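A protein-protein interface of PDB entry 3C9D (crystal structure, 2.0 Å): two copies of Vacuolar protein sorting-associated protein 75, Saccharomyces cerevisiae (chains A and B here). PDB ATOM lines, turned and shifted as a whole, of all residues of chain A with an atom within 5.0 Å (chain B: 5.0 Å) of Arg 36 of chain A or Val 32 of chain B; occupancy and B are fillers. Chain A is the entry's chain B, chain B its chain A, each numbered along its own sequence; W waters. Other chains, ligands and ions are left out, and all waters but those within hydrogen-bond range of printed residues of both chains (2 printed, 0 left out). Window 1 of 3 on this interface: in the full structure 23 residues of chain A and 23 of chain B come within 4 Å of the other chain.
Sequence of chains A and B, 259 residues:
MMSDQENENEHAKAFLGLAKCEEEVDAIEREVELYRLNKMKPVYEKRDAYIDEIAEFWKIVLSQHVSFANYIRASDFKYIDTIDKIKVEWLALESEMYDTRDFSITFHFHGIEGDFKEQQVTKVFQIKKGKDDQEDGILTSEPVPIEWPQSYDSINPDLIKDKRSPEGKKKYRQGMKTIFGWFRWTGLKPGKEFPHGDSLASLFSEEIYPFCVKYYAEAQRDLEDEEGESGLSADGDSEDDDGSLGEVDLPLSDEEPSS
The side-chain carboxylate of Glu 33 of chain B is in salt-bridge range of the guanidinium group of Arg 36 of chain B (2.5 Å).
OE1 of Glu 33 of chain A lies within salt-bridge range of NH1 of Arg 36 of chain A.
Arg 36 of chain A touches just these residues of chain B: Glu 29 and Val 32.
Of the printed residues of chain A, Glu 29 of chain B touches Arg 36.
Printed residues of chain B within 4 Å of Lys 39 of chain A: Ile 28 (3.8 Å) and Glu 31 (3.2 Å).
The nearest residue of chain B that does not touch Arg 36 of chain A is Ile 28 of chain B (4.6 Å).
The side-chain carboxylate (OE2) of Glu 31 of chain B lies within hydrogen-bond range of the side-chain hydroxyl (OH) of Tyr 35 of chain A (2.5 Å).
OE2 of Glu 29 of chain B lies within salt-bridge range of NH2 of Arg 36 of chain A, 2.6 Å away.
The side-chain carboxylate of Glu 31 of chain B lies within salt-bridge range of the side-chain amino group of Lys 39 of chain A.
Val 32 of chain A touches its own counterpart, Val 32 of chain B.
Val 32 of chain A touches Arg 36 of chain B, and with the chains exchanged Arg 36 of chain A touches Val 32 of chain B.
Tyr 35 of chain A touches its own counterpart, Tyr 35 of chain B.
5 positions are printed for both chains.
Of the 9 pairs that touch across the chains among the printed residues, 4 have their exchanged pair printed and touching as well.
Water W2 lies within hydrogen-bond range of the side-chain carboxylate of Glu 29 of chain B, the guanidinium group of Arg 36 of chain A and the side-chain sulfur of Met 40 of chain A.
Water W1 lies within hydrogen-bond range of the side-chain carboxylate of Glu 29 of chain B and the guanidinium group of Arg 36 of chain A.
Among the printed residues, pairs that only touch across the chains: Val 32 of chain A with Val 32 of chain B (3.4 Å), Tyr 35 of chain A with Tyr 35 of chain B (3.6 Å), Met 40 of chain A with Ile 28 of chain B (3.7 Å), Lys 39 of chain A with Ile 28 of chain B (3.8 Å), Arg 36 of chain A with Val 32 of chain B (3.8 Å) and Val 32 of chain A with Arg 36 of chain B (3.8 Å).
Of the 9 printed residues of chain B, 6 touch a printed residue of chain A.
Hydrophobic or aromatic side chains of chain A that line the printed part of chain B: Val 32, Tyr 35 and Met 40.
Among the printed residues, 9 pairs touch across the chains.
Among the printed residues, Asp or Glu carboxylates within 4 Å of a Lys or Arg side-chain nitrogen of the other chain: Arg 36 of chain A with Glu 29 of chain B and Lys 39 of chain A with Glu 31 of chain B.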
ATOM      1  N   VAL A  32      24.903  -2.605  33.620  1.00  0.00           N
ATOM      2  CA  VAL A  32      23.768  -2.307  32.729  1.00  0.00           C
ATOM      3  C   VAL A  32      23.616  -3.333  31.595  1.00  0.00           C
ATOM      4  O   VAL A  32      22.497  -3.760  31.282  1.00  0.00           O
ATOM      5  CB  VAL A  32      23.871  -0.876  32.127  1.00  0.00           C
ATOM      6  CG1 VAL A  32      22.788  -0.650  31.077  1.00  0.00           C
ATOM      7  CG2 VAL A  32      23.780   0.178  33.228  1.00  0.00           C
ATOM      8  N   GLU A  33      24.733  -3.718  30.983  1.00  0.00           N
ATOM      9  CA  GLU A  33      24.702  -4.705  29.897  1.00  0.00           C
ATOM     10  C   GLU A  33      24.313  -6.094  30.415  1.00  0.00           C
ATOM     11  O   GLU A  33      23.562  -6.811  29.762  1.00  0.00           O
ATOM     12  CB  GLU A  33      26.043  -4.743  29.136  1.00  0.00           C
ATOM     13  CG  GLU A  33      26.042  -5.626  27.866  1.00  0.00           C
ATOM     14  CD  GLU A  33      25.012  -5.194  26.796  1.00  0.00           C
ATOM     15  OE1 GLU A  33      24.412  -4.102  26.915  1.00  0.00           O
ATOM     16  OE2 GLU A  33      24.813  -5.957  25.826  1.00  0.00           O
ATOM     17  N   LEU A  34      24.794  -6.454  31.602  1.00  0.00           N
ATOM     18  CA  LEU A  34      24.365  -7.716  32.241  1.00  0.00           C
ATOM     19  C   LEU A  34      22.873  -7.699  32.580  1.00  0.00           C
ATOM     20  O   LEU A  34      22.169  -8.698  32.398  1.00  0.00           O
ATOM     21  CB  LEU A  34      25.200  -8.005  33.489  1.00  0.00           C
ATOM     22  CG  LEU A  34      26.644  -8.448  33.219  1.00  0.00           C
ATOM     23  CD1 LEU A  34      27.431  -8.532  34.515  1.00  0.00           C
ATOM     24  CD2 LEU A  34      26.663  -9.787  32.509  1.00  0.00           C
ATOM     25  N   TYR A  35      22.401  -6.546  33.054  1.00  0.00           N
ATOM     26  CA  TYR A  35      20.981  -6.315  33.316  1.00  0.00           C
ATOM     27  C   TYR A  35      20.186  -6.553  32.023  1.00  0.00           C
ATOM     28  O   TYR A  35      19.235  -7.341  31.997  1.00  0.00           O
ATOM     29  CB  TYR A  35      20.793  -4.879  33.834  1.00  0.00           C
ATOM     30  CG  TYR A  35      19.390  -4.473  34.276  1.00  0.00           C
ATOM     31  CD1 TYR A  35      18.388  -5.415  34.502  1.00  0.00           C
ATOM     32  CD2 TYR A  35      19.089  -3.127  34.516  1.00  0.00           C
ATOM     33  CE1 TYR A  35      17.099  -5.020  34.925  1.00  0.00           C
ATOM     34  CE2 TYR A  35      17.819  -2.726  34.940  1.00  0.00           C
ATOM     35  CZ  TYR A  35      16.834  -3.679  35.144  1.00  0.00           C
ATOM     36  OH  TYR A  35      15.585  -3.280  35.576  1.00  0.00           O
ATOM     37  N   ARG A  36      20.595  -5.879  30.954  1.00  0.00           N
ATOM     38  CA  ARG A  36      19.967  -6.046  29.658  1.00  0.00           C
ATOM     39  C   ARG A  36      19.967  -7.523  29.227  1.00  0.00           C
ATOM     40  O   ARG A  36      18.924  -8.071  28.862  1.00  0.00           O
ATOM     41  CB  ARG A  36      20.679  -5.179  28.620  1.00  0.00           C
ATOM     42  CG  ARG A  36      19.984  -5.097  27.272  1.00  0.00           C
ATOM     43  CD  ARG A  36      20.884  -4.399  26.257  1.00  0.00           C
ATOM     44  NE  ARG A  36      20.265  -4.316  24.939  1.00  0.00           N
ATOM     45  CZ  ARG A  36      20.851  -3.799  23.861  1.00  0.00           C
ATOM     46  NH1 ARG A  36      22.088  -3.314  23.933  1.00  0.00           N
ATOM     47  NH2 ARG A  36      20.203  -3.767  22.706  1.00  0.00           N
ATOM     48  N   LEU A  37      21.134  -8.161  29.278  1.00  0.00           N
ATOM     49  CA  LEU A  37      21.281  -9.520  28.746  1.00  0.00           C
ATOM     50  C   LEU A  37      20.449 -10.557  29.528  1.00  0.00           C
ATOM     51  O   LEU A  37      19.872 -11.474  28.931  1.00  0.00           O
ATOM     52  CB  LEU A  37      22.760  -9.932  28.688  1.00  0.00           C
ATOM     53  CG  LEU A  37      23.671  -9.255  27.642  1.00  0.00           C
ATOM     54  CD1 LEU A  37      25.124  -9.596  27.902  1.00  0.00           C
ATOM     55  CD2 LEU A  37      23.281  -9.606  26.194  1.00  0.00           C
ATOM     56  N   ASN A  38      20.380 -10.397  30.853  1.00  0.00           N
ATOM     57  CA  ASN A  38      19.589 -11.310  31.696  1.00  0.00           C
ATOM     58  C   ASN A  38      18.097 -11.191  31.411  1.00  0.00           C
ATOM     59  O   ASN A  38      17.390 -12.197  31.287  1.00  0.00           O
ATOM     60  CB  ASN A  38      19.870 -11.073  33.189  1.00  0.00           C
ATOM     61  CG  ASN A  38      21.114 -11.806  33.672  1.00  0.00           C
ATOM     62  OD1 ASN A  38      21.147 -13.042  33.722  1.00  0.00           O
ATOM     63  ND2 ASN A  38      22.137 -11.052  34.032  1.00  0.00           N
ATOM     64  N   LYS A  39      17.626  -9.957  31.269  1.00  0.00           N
ATOM     65  CA  LYS A  39      16.236  -9.712  30.935  1.00  0.00           C
ATOM     66  C   LYS A  39      15.891 -10.224  29.521  1.00  0.00           C
ATOM     67  O   LYS A  39      14.783 -10.720  29.283  1.00  0.00           O
ATOM     68  CB  LYS A  39      15.916  -8.221  31.080  1.00  0.00           C
ATOM     69  CG  LYS A  39      14.768  -7.964  32.007  1.00  0.00           C
ATOM     70  CD  LYS A  39      14.455  -6.494  32.189  1.00  0.00           C
ATOM     71  CE  LYS A  39      12.993  -6.328  32.527  1.00  0.00           C
ATOM     72  NZ  LYS A  39      12.583  -7.115  33.738  1.00  0.00           N
ATOM     73  N   MET A  40      16.856 -10.139  28.606  1.00  0.00           N
ATOM     74  CA  MET A  40      16.648 -10.544  27.207  1.00  0.00           C
ATOM     75  C   MET A  40      16.610 -12.053  26.995  1.00  0.00           C
ATOM     76  O   MET A  40      16.035 -12.523  26.019  1.00  0.00           O
ATOM     77  CB  MET A  40      17.720  -9.929  26.291  1.00  0.00           C
ATOM     78  CG  MET A  40      17.486  -8.478  25.943  1.00  0.00           C
ATOM     79  SD  MET A  40      15.905  -8.171  25.133  1.00  0.00           S
ATOM     80  CE  MET A  40      15.946  -9.382  23.808  1.00  0.00           C
ATOM     81  N   PHE A 211      18.826  -7.993  15.970  1.00  0.00           N
ATOM     82  CA  PHE A 211      17.879  -7.233  15.164  1.00  0.00           C
ATOM     83  C   PHE A 211      17.348  -7.980  13.929  1.00  0.00           C
ATOM     84  O   PHE A 211      16.759  -7.367  13.035  1.00  0.00           O
ATOM     85  CB  PHE A 211      18.488  -5.877  14.766  1.00  0.00           C
ATOM     86  CG  PHE A 211      18.973  -5.057  15.940  1.00  0.00           C
ATOM     87  CD1 PHE A 211      18.110  -4.735  16.990  1.00  0.00           C
ATOM     88  CD2 PHE A 211      20.281  -4.599  15.987  1.00  0.00           C
ATOM     89  CE1 PHE A 211      18.561  -3.975  18.081  1.00  0.00           C
ATOM     90  CE2 PHE A 211      20.735  -3.834  17.068  1.00  0.00           C
ATOM     91  CZ  PHE A 211      19.873  -3.529  18.114  1.00  0.00           C
ATOM     92  N   ILE B  28      11.916  -3.564  27.695  1.00  0.00           N
ATOM     93  CA  ILE B  28      13.211  -3.826  28.325  1.00  0.00           C
ATOM     94  C   ILE B  28      14.220  -2.688  28.114  1.00  0.00           C
ATOM     95  O   ILE B  28      14.886  -2.267  29.063  1.00  0.00           O
ATOM     96  CB  ILE B  28      13.823  -5.179  27.869  1.00  0.00           C
ATOM     97  CG1 ILE B  28      12.988  -6.346  28.405  1.00  0.00           C
ATOM     98  CG2 ILE B  28      15.280  -5.303  28.336  1.00  0.00           C
ATOM     99  CD1 ILE B  28      13.229  -7.674  27.668  1.00  0.00           C
ATOM    100  N   GLU B  29      14.329  -2.193  26.878  1.00  0.00           N
ATOM    101  CA  GLU B  29      15.301  -1.141  26.562  1.00  0.00           C
ATOM    102  C   GLU B  29      15.038   0.116  27.394  1.00  0.00           C
ATOM    103  O   GLU B  29      15.969   0.759  27.859  1.00  0.00           O
ATOM    104  CB  GLU B  29      15.289  -0.794  25.066  1.00  0.00           C
ATOM    105  CG  GLU B  29      15.855  -1.873  24.141  1.00  0.00           C
ATOM    106  CD  GLU B  29      17.383  -1.967  24.150  1.00  0.00           C
ATOM    107  OE1 GLU B  29      18.037  -1.380  25.042  1.00  0.00           O
ATOM    108  OE2 GLU B  29      17.938  -2.650  23.253  1.00  0.00           O
ATOM    109  N   ARG B  30      13.765   0.450  27.580  1.00  0.00           N
ATOM    110  CA  ARG B  30      13.393   1.586  28.421  1.00  0.00           C
ATOM    111  C   ARG B  30      13.817   1.379  29.884  1.00  0.00           C
ATOM    112  O   ARG B  30      14.456   2.252  30.483  1.00  0.00           O
ATOM    113  CB  ARG B  30      11.889   1.871  28.336  1.00  0.00           C
ATOM    114  CG  ARG B  30      11.512   3.161  29.040  1.00  0.00           C
ATOM    115  CD  ARG B  30      10.026   3.322  29.253  1.00  0.00           C
ATOM    116  NE  ARG B  30       9.780   4.226  30.381  1.00  0.00           N
ATOM    117  CZ  ARG B  30       9.869   5.558  30.324  1.00  0.00           C
ATOM    118  NH1 ARG B  30      10.177   6.173  29.188  1.00  0.00           N
ATOM    119  NH2 ARG B  30       9.648   6.277  31.415  1.00  0.00           N
ATOM    120  N   GLU B  31      13.453   0.227  30.447  1.00  0.00           N
ATOM    121  CA  GLU B  31      13.789  -0.103  31.841  1.00  0.00           C
ATOM    122  C   GLU B  31      15.301  -0.065  32.076  1.00  0.00           C
ATOM    123  O   GLU B  31      15.770   0.478  33.076  1.00  0.00           O
ATOM    124  CB  GLU B  31      13.203  -1.472  32.236  1.00  0.00           C
ATOM    125  CG  GLU B  31      13.691  -2.007  33.589  1.00  0.00           C
ATOM    126  CD  GLU B  31      12.793  -3.108  34.174  1.00  0.00           C
ATOM    127  OE1 GLU B  31      11.553  -3.017  34.030  1.00  0.00           O
ATOM    128  OE2 GLU B  31      13.335  -4.055  34.796  1.00  0.00           O
ATOM    129  N   VAL B  32      16.058  -0.633  31.144  1.00  0.00           N
ATOM    130  CA  VAL B  32      17.515  -0.654  31.241  1.00  0.00           C
ATOM    131  C   VAL B  32      18.085   0.769  31.155  1.00  0.00           C
ATOM    132  O   VAL B  32      18.948   1.142  31.946  1.00  0.00           O
ATOM    133  CB  VAL B  32      18.151  -1.570  30.154  1.00  0.00           C
ATOM    134  CG1 VAL B  32      19.650  -1.434  30.139  1.00  0.00           C
ATOM    135  CG2 VAL B  32      17.762  -3.026  30.396  1.00  0.00           C
ATOM    136  N   GLU B  33      17.590   1.561  30.204  1.00  0.00           N
ATOM    137  CA  GLU B  33      18.067   2.936  30.042  1.00  0.00           C
ATOM    138  C   GLU B  33      17.756   3.802  31.272  1.00  0.00           C
ATOM    139  O   GLU B  33      18.610   4.561  31.730  1.00  0.00           O
ATOM    140  CB  GLU B  33      17.508   3.570  28.765  1.00  0.00           C
ATOM    141  CG  GLU B  33      17.985   5.011  28.507  1.00  0.00           C
ATOM    142  CD  GLU B  33      19.495   5.130  28.318  1.00  0.00           C
ATOM    143  OE1 GLU B  33      20.179   4.088  28.196  1.00  0.00           O
ATOM    144  OE2 GLU B  33      19.993   6.276  28.276  1.00  0.00           O
ATOM    145  N   LEU B  34      16.548   3.658  31.819  1.00  0.00           N
ATOM    146  CA  LEU B  34      16.177   4.362  33.054  1.00  0.00           C
ATOM    147  C   LEU B  34      17.145   4.069  34.198  1.00  0.00           C
ATOM    148  O   LEU B  34      17.568   4.985  34.915  1.00  0.00           O
ATOM    149  CB  LEU B  34      14.753   4.010  33.484  1.00  0.00           C
ATOM    150  CG  LEU B  34      13.598   4.671  32.733  1.00  0.00           C
ATOM    151  CD1 LEU B  34      12.264   4.033  33.135  1.00  0.00           C
ATOM    152  CD2 LEU B  34      13.572   6.165  32.982  1.00  0.00           C
ATOM    153  N   TYR B  35      17.479   2.789  34.363  1.00  0.00           N
ATOM    154  CA  TYR B  35      18.447   2.337  35.368  1.00  0.00           C
ATOM    155  C   TYR B  35      19.842   2.933  35.138  1.00  0.00           C
ATOM    156  O   TYR B  35      20.484   3.403  36.077  1.00  0.00           O
ATOM    157  CB  TYR B  35      18.521   0.804  35.383  1.00  0.00           C
ATOM    158  CG  TYR B  35      19.368   0.233  36.506  1.00  0.00           C
ATOM    159  CD1 TYR B  35      18.889   0.200  37.817  1.00  0.00           C
ATOM    160  CD2 TYR B  35      20.637  -0.280  36.257  1.00  0.00           C
ATOM    161  CE1 TYR B  35      19.656  -0.318  38.849  1.00  0.00           C
ATOM    162  CE2 TYR B  35      21.414  -0.807  37.284  1.00  0.00           C
ATOM    163  CZ  TYR B  35      20.914  -0.825  38.578  1.00  0.00           C
ATOM    164  OH  TYR B  35      21.669  -1.342  39.607  1.00  0.00           O
ATOM    165  N   ARG B  36      20.304   2.897  33.885  1.00  0.00           N
ATOM    166  CA  ARG B  36      21.590   3.483  33.509  1.00  0.00           C
ATOM    167  C   ARG B  36      21.648   4.977  33.848  1.00  0.00           C
ATOM    168  O   ARG B  36      22.624   5.449  34.429  1.00  0.00           O
ATOM    169  CB  ARG B  36      21.850   3.268  32.017  1.00  0.00           C
ATOM    170  CG  ARG B  36      23.125   3.918  31.473  1.00  0.00           C
ATOM    171  CD  ARG B  36      23.164   3.760  29.947  1.00  0.00           C
ATOM    172  NE  ARG B  36      23.492   4.996  29.231  1.00  0.00           N
ATOM    173  CZ  ARG B  36      22.797   6.133  29.308  1.00  0.00           C
ATOM    174  NH1 ARG B  36      21.737   6.230  30.104  1.00  0.00           N
ATOM    175  NH2 ARG B  36      23.168   7.185  28.592  1.00  0.00           N
HETATM  176  O   HOH W   1      18.915  -1.624  20.688  1.00  0.00           O
HETATM  177  O   HOH W   2      17.828  -5.474  23.527  1.00  0.00           O
